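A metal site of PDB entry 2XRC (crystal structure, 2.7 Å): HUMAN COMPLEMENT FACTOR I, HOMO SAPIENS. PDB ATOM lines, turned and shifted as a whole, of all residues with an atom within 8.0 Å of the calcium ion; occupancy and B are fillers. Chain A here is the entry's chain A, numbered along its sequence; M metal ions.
Six residues have an atom within 4 Å of the calcium ion: Lys 221, Asp 224, Ile 226, Asp 228, Asp 234 and Glu 235.
The nearest printed residue that does not touch the calcium ion is Cys 223 (4.2 Å).
N of Cys 223 lies close to OE2 of Glu 235 (3.4 Å).
The backbone NH (N) of Gly 225 sits at hydrogen-bond distance from the side-chain carboxylate (OE1) of Glu 235, 2.6 Å away.
O of Glu 235 is in hydrogen-bond range of N of Cys 253 (3.1 Å).
O of Asp 234 sits at hydrogen-bond distance from N of Cys 223 (2.7 Å).
N of Asp 234 sits close to SG of Cys 229, at 3.6 Å.
SG of Cys 223 forms a disulfide with SG of Cys 238, 2.0 Å away.
The calcium ion is bound by O of Lys 221, 2.3 Å away.
OE2 of Glu 235 is bound to the calcium ion (2.3 Å).
The calcium ion is bound by OD1 of Asp 234 (2.4 Å).
O of Ile 226 binds the calcium ion (2.5 Å).
OD1 of Asp 224 binds the calcium ion (2.5 Å).
The calcium ion is bound by OD2 of Asp 228 (2.6 Å).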
ATOM      1  N   MET A 129      -7.331   7.595  28.962  1.00  0.00           N
ATOM      2  CA  MET A 129      -7.350   6.313  29.666  1.00  0.00           C
ATOM      3  C   MET A 129      -6.076   5.486  29.453  1.00  0.00           C
ATOM      4  O   MET A 129      -5.719   4.671  30.309  1.00  0.00           O
ATOM      5  CB  MET A 129      -8.564   5.479  29.234  1.00  0.00           C
ATOM      6  CG  MET A 129      -9.889   5.952  29.806  1.00  0.00           C
ATOM      7  SD  MET A 129     -10.090   5.655  31.571  1.00  0.00           S
ATOM      8  CE  MET A 129      -9.900   7.330  32.194  1.00  0.00           C
ATOM      9  N   THR A 147     -13.427   5.579  34.875  1.00  0.00           N
ATOM     10  CA  THR A 147     -13.874   6.246  33.658  1.00  0.00           C
ATOM     11  C   THR A 147     -15.070   7.170  33.917  1.00  0.00           C
ATOM     12  O   THR A 147     -15.232   8.191  33.240  1.00  0.00           O
ATOM     13  CB  THR A 147     -14.287   5.205  32.615  1.00  0.00           C
ATOM     14  OG1 THR A 147     -15.345   4.399  33.129  1.00  0.00           O
ATOM     15  CG2 THR A 147     -13.112   4.306  32.280  1.00  0.00           C
ATOM     16  N   PHE A 209     -20.991  -2.112  30.357  1.00  0.00           N
ATOM     17  CA  PHE A 209     -20.019  -3.122  29.938  1.00  0.00           C
ATOM     18  C   PHE A 209     -19.057  -3.468  31.071  1.00  0.00           C
ATOM     19  O   PHE A 209     -18.381  -2.584  31.610  1.00  0.00           O
ATOM     20  CB  PHE A 209     -19.221  -2.629  28.727  1.00  0.00           C
ATOM     21  CG  PHE A 209     -18.398  -3.700  28.054  1.00  0.00           C
ATOM     22  CD1 PHE A 209     -18.956  -4.486  27.054  1.00  0.00           C
ATOM     23  CD2 PHE A 209     -17.080  -3.927  28.436  1.00  0.00           C
ATOM     24  CE1 PHE A 209     -18.206  -5.479  26.441  1.00  0.00           C
ATOM     25  CE2 PHE A 209     -16.326  -4.924  27.830  1.00  0.00           C
ATOM     26  CZ  PHE A 209     -16.895  -5.698  26.831  1.00  0.00           C
ATOM     27  N   ILE A 217     -17.819  -0.492  33.407  1.00  0.00           N
ATOM     28  CA  ILE A 217     -17.875   0.815  32.735  1.00  0.00           C
ATOM     29  C   ILE A 217     -19.207   0.938  32.011  1.00  0.00           C
ATOM     30  O   ILE A 217     -19.903  -0.048  31.823  1.00  0.00           O
ATOM     31  CB  ILE A 217     -16.713   1.014  31.729  1.00  0.00           C
ATOM     32  CG1 ILE A 217     -16.596  -0.166  30.764  1.00  0.00           C
ATOM     33  CG2 ILE A 217     -15.396   1.208  32.468  1.00  0.00           C
ATOM     34  CD1 ILE A 217     -15.737   0.118  29.546  1.00  0.00           C
ATOM     35  N   SER A 218     -19.549   2.158  31.622  1.00  0.00           N
ATOM     36  CA  SER A 218     -20.796   2.410  30.894  1.00  0.00           C
ATOM     37  C   SER A 218     -20.705   1.862  29.473  1.00  0.00           C
ATOM     38  O   SER A 218     -19.603   1.707  28.933  1.00  0.00           O
ATOM     39  CB  SER A 218     -21.127   3.900  30.875  1.00  0.00           C
ATOM     40  OG  SER A 218     -22.437   4.119  30.382  1.00  0.00           O
ATOM     41  N   GLN A 219     -21.856   1.590  28.864  1.00  0.00           N
ATOM     42  CA  GLN A 219     -21.927   0.938  27.555  1.00  0.00           C
ATOM     43  C   GLN A 219     -21.491   1.855  26.401  1.00  0.00           C
ATOM     44  O   GLN A 219     -21.147   1.377  25.318  1.00  0.00           O
ATOM     45  CB  GLN A 219     -23.340   0.410  27.302  1.00  0.00           C
ATOM     46  CG  GLN A 219     -23.464  -0.633  26.181  1.00  0.00           C
ATOM     47  CD  GLN A 219     -22.986  -2.027  26.576  1.00  0.00           C
ATOM     48  OE1 GLN A 219     -22.365  -2.213  27.623  1.00  0.00           O
ATOM     49  NE2 GLN A 219     -23.268  -3.012  25.731  1.00  0.00           N
ATOM     50  N   MET A 220     -21.525   3.166  26.636  1.00  0.00           N
ATOM     51  CA  MET A 220     -21.117   4.149  25.623  1.00  0.00           C
ATOM     52  C   MET A 220     -19.595   4.129  25.375  1.00  0.00           C
ATOM     53  O   MET A 220     -19.135   4.537  24.313  1.00  0.00           O
ATOM     54  CB  MET A 220     -21.546   5.562  26.039  1.00  0.00           C
ATOM     55  CG  MET A 220     -23.059   5.752  26.170  1.00  0.00           C
ATOM     56  SD  MET A 220     -23.942   5.720  24.594  1.00  0.00           S
ATOM     57  CE  MET A 220     -25.564   6.306  25.093  1.00  0.00           C
ATOM     58  N   LYS A 221     -18.844   3.652  26.368  1.00  0.00           N
ATOM     59  CA  LYS A 221     -17.386   3.513  26.245  1.00  0.00           C
ATOM     60  C   LYS A 221     -16.998   2.241  25.496  1.00  0.00           C
ATOM     61  O   LYS A 221     -15.882   2.136  24.963  1.00  0.00           O
ATOM     62  CB  LYS A 221     -16.725   3.509  27.623  1.00  0.00           C
ATOM     63  CG  LYS A 221     -16.967   4.774  28.450  1.00  0.00           C
ATOM     64  CD  LYS A 221     -16.301   5.988  27.835  1.00  0.00           C
ATOM     65  CE  LYS A 221     -16.375   7.193  28.775  1.00  0.00           C
ATOM     66  NZ  LYS A 221     -15.706   8.386  28.186  1.00  0.00           N
ATOM     67  N   ALA A 222     -17.904   1.261  25.445  1.00  0.00           N
ATOM     68  CA  ALA A 222     -17.641  -0.012  24.780  1.00  0.00           C
ATOM     69  C   ALA A 222     -17.531   0.135  23.254  1.00  0.00           C
ATOM     70  O   ALA A 222     -18.348   0.820  22.630  1.00  0.00           O
ATOM     71  CB  ALA A 222     -18.727  -1.016  25.125  1.00  0.00           C
ATOM     72  N   CYS A 223     -16.514  -0.494  22.672  1.00  0.00           N
ATOM     73  CA  CYS A 223     -16.272  -0.498  21.229  1.00  0.00           C
ATOM     74  C   CYS A 223     -16.168   0.913  20.625  1.00  0.00           C
ATOM     75  O   CYS A 223     -16.972   1.281  19.756  1.00  0.00           O
ATOM     76  CB  CYS A 223     -17.344  -1.309  20.499  1.00  0.00           C
ATOM     77  SG  CYS A 223     -17.338  -3.080  20.884  1.00  0.00           S
ATOM     78  N   ASP A 224     -15.184   1.697  21.072  1.00  0.00           N
ATOM     79  CA  ASP A 224     -14.907   3.022  20.486  1.00  0.00           C
ATOM     80  C   ASP A 224     -13.446   3.231  20.041  1.00  0.00           C
ATOM     81  O   ASP A 224     -13.086   4.327  19.588  1.00  0.00           O
ATOM     82  CB  ASP A 224     -15.342   4.145  21.449  1.00  0.00           C
ATOM     83  CG  ASP A 224     -14.662   4.083  22.797  1.00  0.00           C
ATOM     84  OD1 ASP A 224     -13.768   3.225  22.989  1.00  0.00           O
ATOM     85  OD2 ASP A 224     -15.034   4.882  23.687  1.00  0.00           O
ATOM     86  N   GLY A 225     -12.623   2.199  20.154  1.00  0.00           N
ATOM     87  CA  GLY A 225     -11.205   2.272  19.787  1.00  0.00           C
ATOM     88  C   GLY A 225     -10.273   2.497  20.968  1.00  0.00           C
ATOM     89  O   GLY A 225      -9.074   2.236  20.864  1.00  0.00           O
ATOM     90  N   ILE A 226     -10.822   2.994  22.077  1.00  0.00           N
ATOM     91  CA  ILE A 226     -10.040   3.294  23.282  1.00  0.00           C
ATOM     92  C   ILE A 226     -10.107   2.150  24.280  1.00  0.00           C
ATOM     93  O   ILE A 226     -11.186   1.669  24.613  1.00  0.00           O
ATOM     94  CB  ILE A 226     -10.569   4.560  23.982  1.00  0.00           C
ATOM     95  CG1 ILE A 226     -10.615   5.750  23.011  1.00  0.00           C
ATOM     96  CG2 ILE A 226      -9.707   4.890  25.210  1.00  0.00           C
ATOM     97  CD1 ILE A 226     -11.136   7.020  23.644  1.00  0.00           C
ATOM     98  N   ASN A 227      -8.939   1.728  24.769  1.00  0.00           N
ATOM     99  CA  ASN A 227      -8.840   0.769  25.874  1.00  0.00           C
ATOM    100  C   ASN A 227      -9.190   1.459  27.190  1.00  0.00           C
ATOM    101  O   ASN A 227      -8.339   2.081  27.818  1.00  0.00           O
ATOM    102  CB  ASN A 227      -7.415   0.196  25.929  1.00  0.00           C
ATOM    103  CG  ASN A 227      -7.252  -0.882  26.997  1.00  0.00           C
ATOM    104  OD1 ASN A 227      -8.168  -1.157  27.781  1.00  0.00           O
ATOM    105  ND2 ASN A 227      -6.077  -1.497  27.032  1.00  0.00           N
ATOM    106  N   ASP A 228     -10.451   1.343  27.609  1.00  0.00           N
ATOM    107  CA  ASP A 228     -10.894   1.836  28.909  1.00  0.00           C
ATOM    108  C   ASP A 228     -10.638   0.785  30.001  1.00  0.00           C
ATOM    109  O   ASP A 228     -10.469   1.132  31.177  1.00  0.00           O
ATOM    110  CB  ASP A 228     -12.391   2.197  28.895  1.00  0.00           C
ATOM    111  CG  ASP A 228     -12.711   3.371  27.983  1.00  0.00           C
ATOM    112  OD1 ASP A 228     -12.911   4.493  28.504  1.00  0.00           O
ATOM    113  OD2 ASP A 228     -12.770   3.171  26.748  1.00  0.00           O
ATOM    114  N   CYS A 229     -10.625  -0.487  29.608  1.00  0.00           N
ATOM    115  CA  CYS A 229     -10.549  -1.595  30.556  1.00  0.00           C
ATOM    116  C   CYS A 229      -9.168  -1.806  31.177  1.00  0.00           C
ATOM    117  O   CYS A 229      -9.046  -2.034  32.373  1.00  0.00           O
ATOM    118  CB  CYS A 229     -11.010  -2.896  29.883  1.00  0.00           C
ATOM    119  SG  CYS A 229     -12.799  -3.018  29.659  1.00  0.00           S
ATOM    120  N   SER A 233     -11.033  -5.571  26.975  1.00  0.00           N
ATOM    121  CA  SER A 233     -12.273  -6.346  26.934  1.00  0.00           C
ATOM    122  C   SER A 233     -13.309  -5.585  26.107  1.00  0.00           C
ATOM    123  O   SER A 233     -14.053  -6.172  25.322  1.00  0.00           O
ATOM    124  CB  SER A 233     -12.809  -6.568  28.346  1.00  0.00           C
ATOM    125  OG  SER A 233     -11.884  -7.293  29.141  1.00  0.00           O
ATOM    126  N   ASP A 234     -13.325  -4.269  26.271  1.00  0.00           N
ATOM    127  CA  ASP A 234     -14.320  -3.407  25.628  1.00  0.00           C
ATOM    128  C   ASP A 234     -14.090  -3.157  24.140  1.00  0.00           C
ATOM    129  O   ASP A 234     -14.865  -2.434  23.513  1.00  0.00           O
ATOM    130  CB  ASP A 234     -14.442  -2.071  26.387  1.00  0.00           C
ATOM    131  CG  ASP A 234     -13.107  -1.328  26.535  1.00  0.00           C
ATOM    132  OD1 ASP A 234     -13.105  -0.074  26.501  1.00  0.00           O
ATOM    133  OD2 ASP A 234     -12.068  -1.993  26.672  1.00  0.00           O
ATOM    134  N   GLU A 235     -13.048  -3.749  23.564  1.00  0.00           N
ATOM    135  CA  GLU A 235     -12.662  -3.484  22.173  1.00  0.00           C
ATOM    136  C   GLU A 235     -12.550  -4.727  21.279  1.00  0.00           C
ATOM    137  O   GLU A 235     -12.502  -4.586  20.053  1.00  0.00           O
ATOM    138  CB  GLU A 235     -11.340  -2.724  22.133  1.00  0.00           C
ATOM    139  CG  GLU A 235     -11.301  -1.501  23.031  1.00  0.00           C
ATOM    140  CD  GLU A 235     -12.339  -0.470  22.632  1.00  0.00           C
ATOM    141  OE1 GLU A 235     -12.266   0.057  21.500  1.00  0.00           O
ATOM    142  OE2 GLU A 235     -13.228  -0.162  23.464  1.00  0.00           O
ATOM    143  N   CYS A 238     -16.436  -6.516  18.828  1.00  0.00           N
ATOM    144  CA  CYS A 238     -17.103  -5.381  18.197  1.00  0.00           C
ATOM    145  C   CYS A 238     -17.475  -5.657  16.743  1.00  0.00           C
ATOM    146  O   CYS A 238     -16.606  -5.889  15.900  1.00  0.00           O
ATOM    147  CB  CYS A 238     -16.210  -4.137  18.284  1.00  0.00           C
ATOM    148  SG  CYS A 238     -15.660  -3.750  19.963  1.00  0.00           S
ATOM    149  N   GLN A 242     -17.668   2.632  17.499  1.00  0.00           N
ATOM    150  CA  GLN A 242     -18.539   3.740  17.901  1.00  0.00           C
ATOM    151  C   GLN A 242     -18.086   5.040  17.238  1.00  0.00           C
ATOM    152  O   GLN A 242     -18.678   5.478  16.261  1.00  0.00           O
ATOM    153  CB  GLN A 242     -18.562   3.870  19.438  1.00  0.00           C
ATOM    154  CG  GLN A 242     -19.350   5.058  19.976  1.00  0.00           C
ATOM    155  CD  GLN A 242     -20.819   5.020  19.614  1.00  0.00           C
ATOM    156  OE1 GLN A 242     -21.399   3.940  19.462  1.00  0.00           O
ATOM    157  NE2 GLN A 242     -21.426   6.191  19.464  1.00  0.00           N
ATOM    158  N   CYS A 253     -11.720  -3.227  17.347  1.00  0.00           N
ATOM    159  CA  CYS A 253     -11.536  -1.816  16.989  1.00  0.00           C
ATOM    160  C   CYS A 253     -10.117  -1.350  17.332  1.00  0.00           C
ATOM    161  O   CYS A 253      -9.538  -1.793  18.327  1.00  0.00           O
ATOM    162  CB  CYS A 253     -12.559  -0.941  17.721  1.00  0.00           C
ATOM    163  SG  CYS A 253     -14.242  -1.024  17.074  1.00  0.00           S
HETATM  164 CA    CA M   1     -13.626   1.658  24.873  1.00  0.00          CA
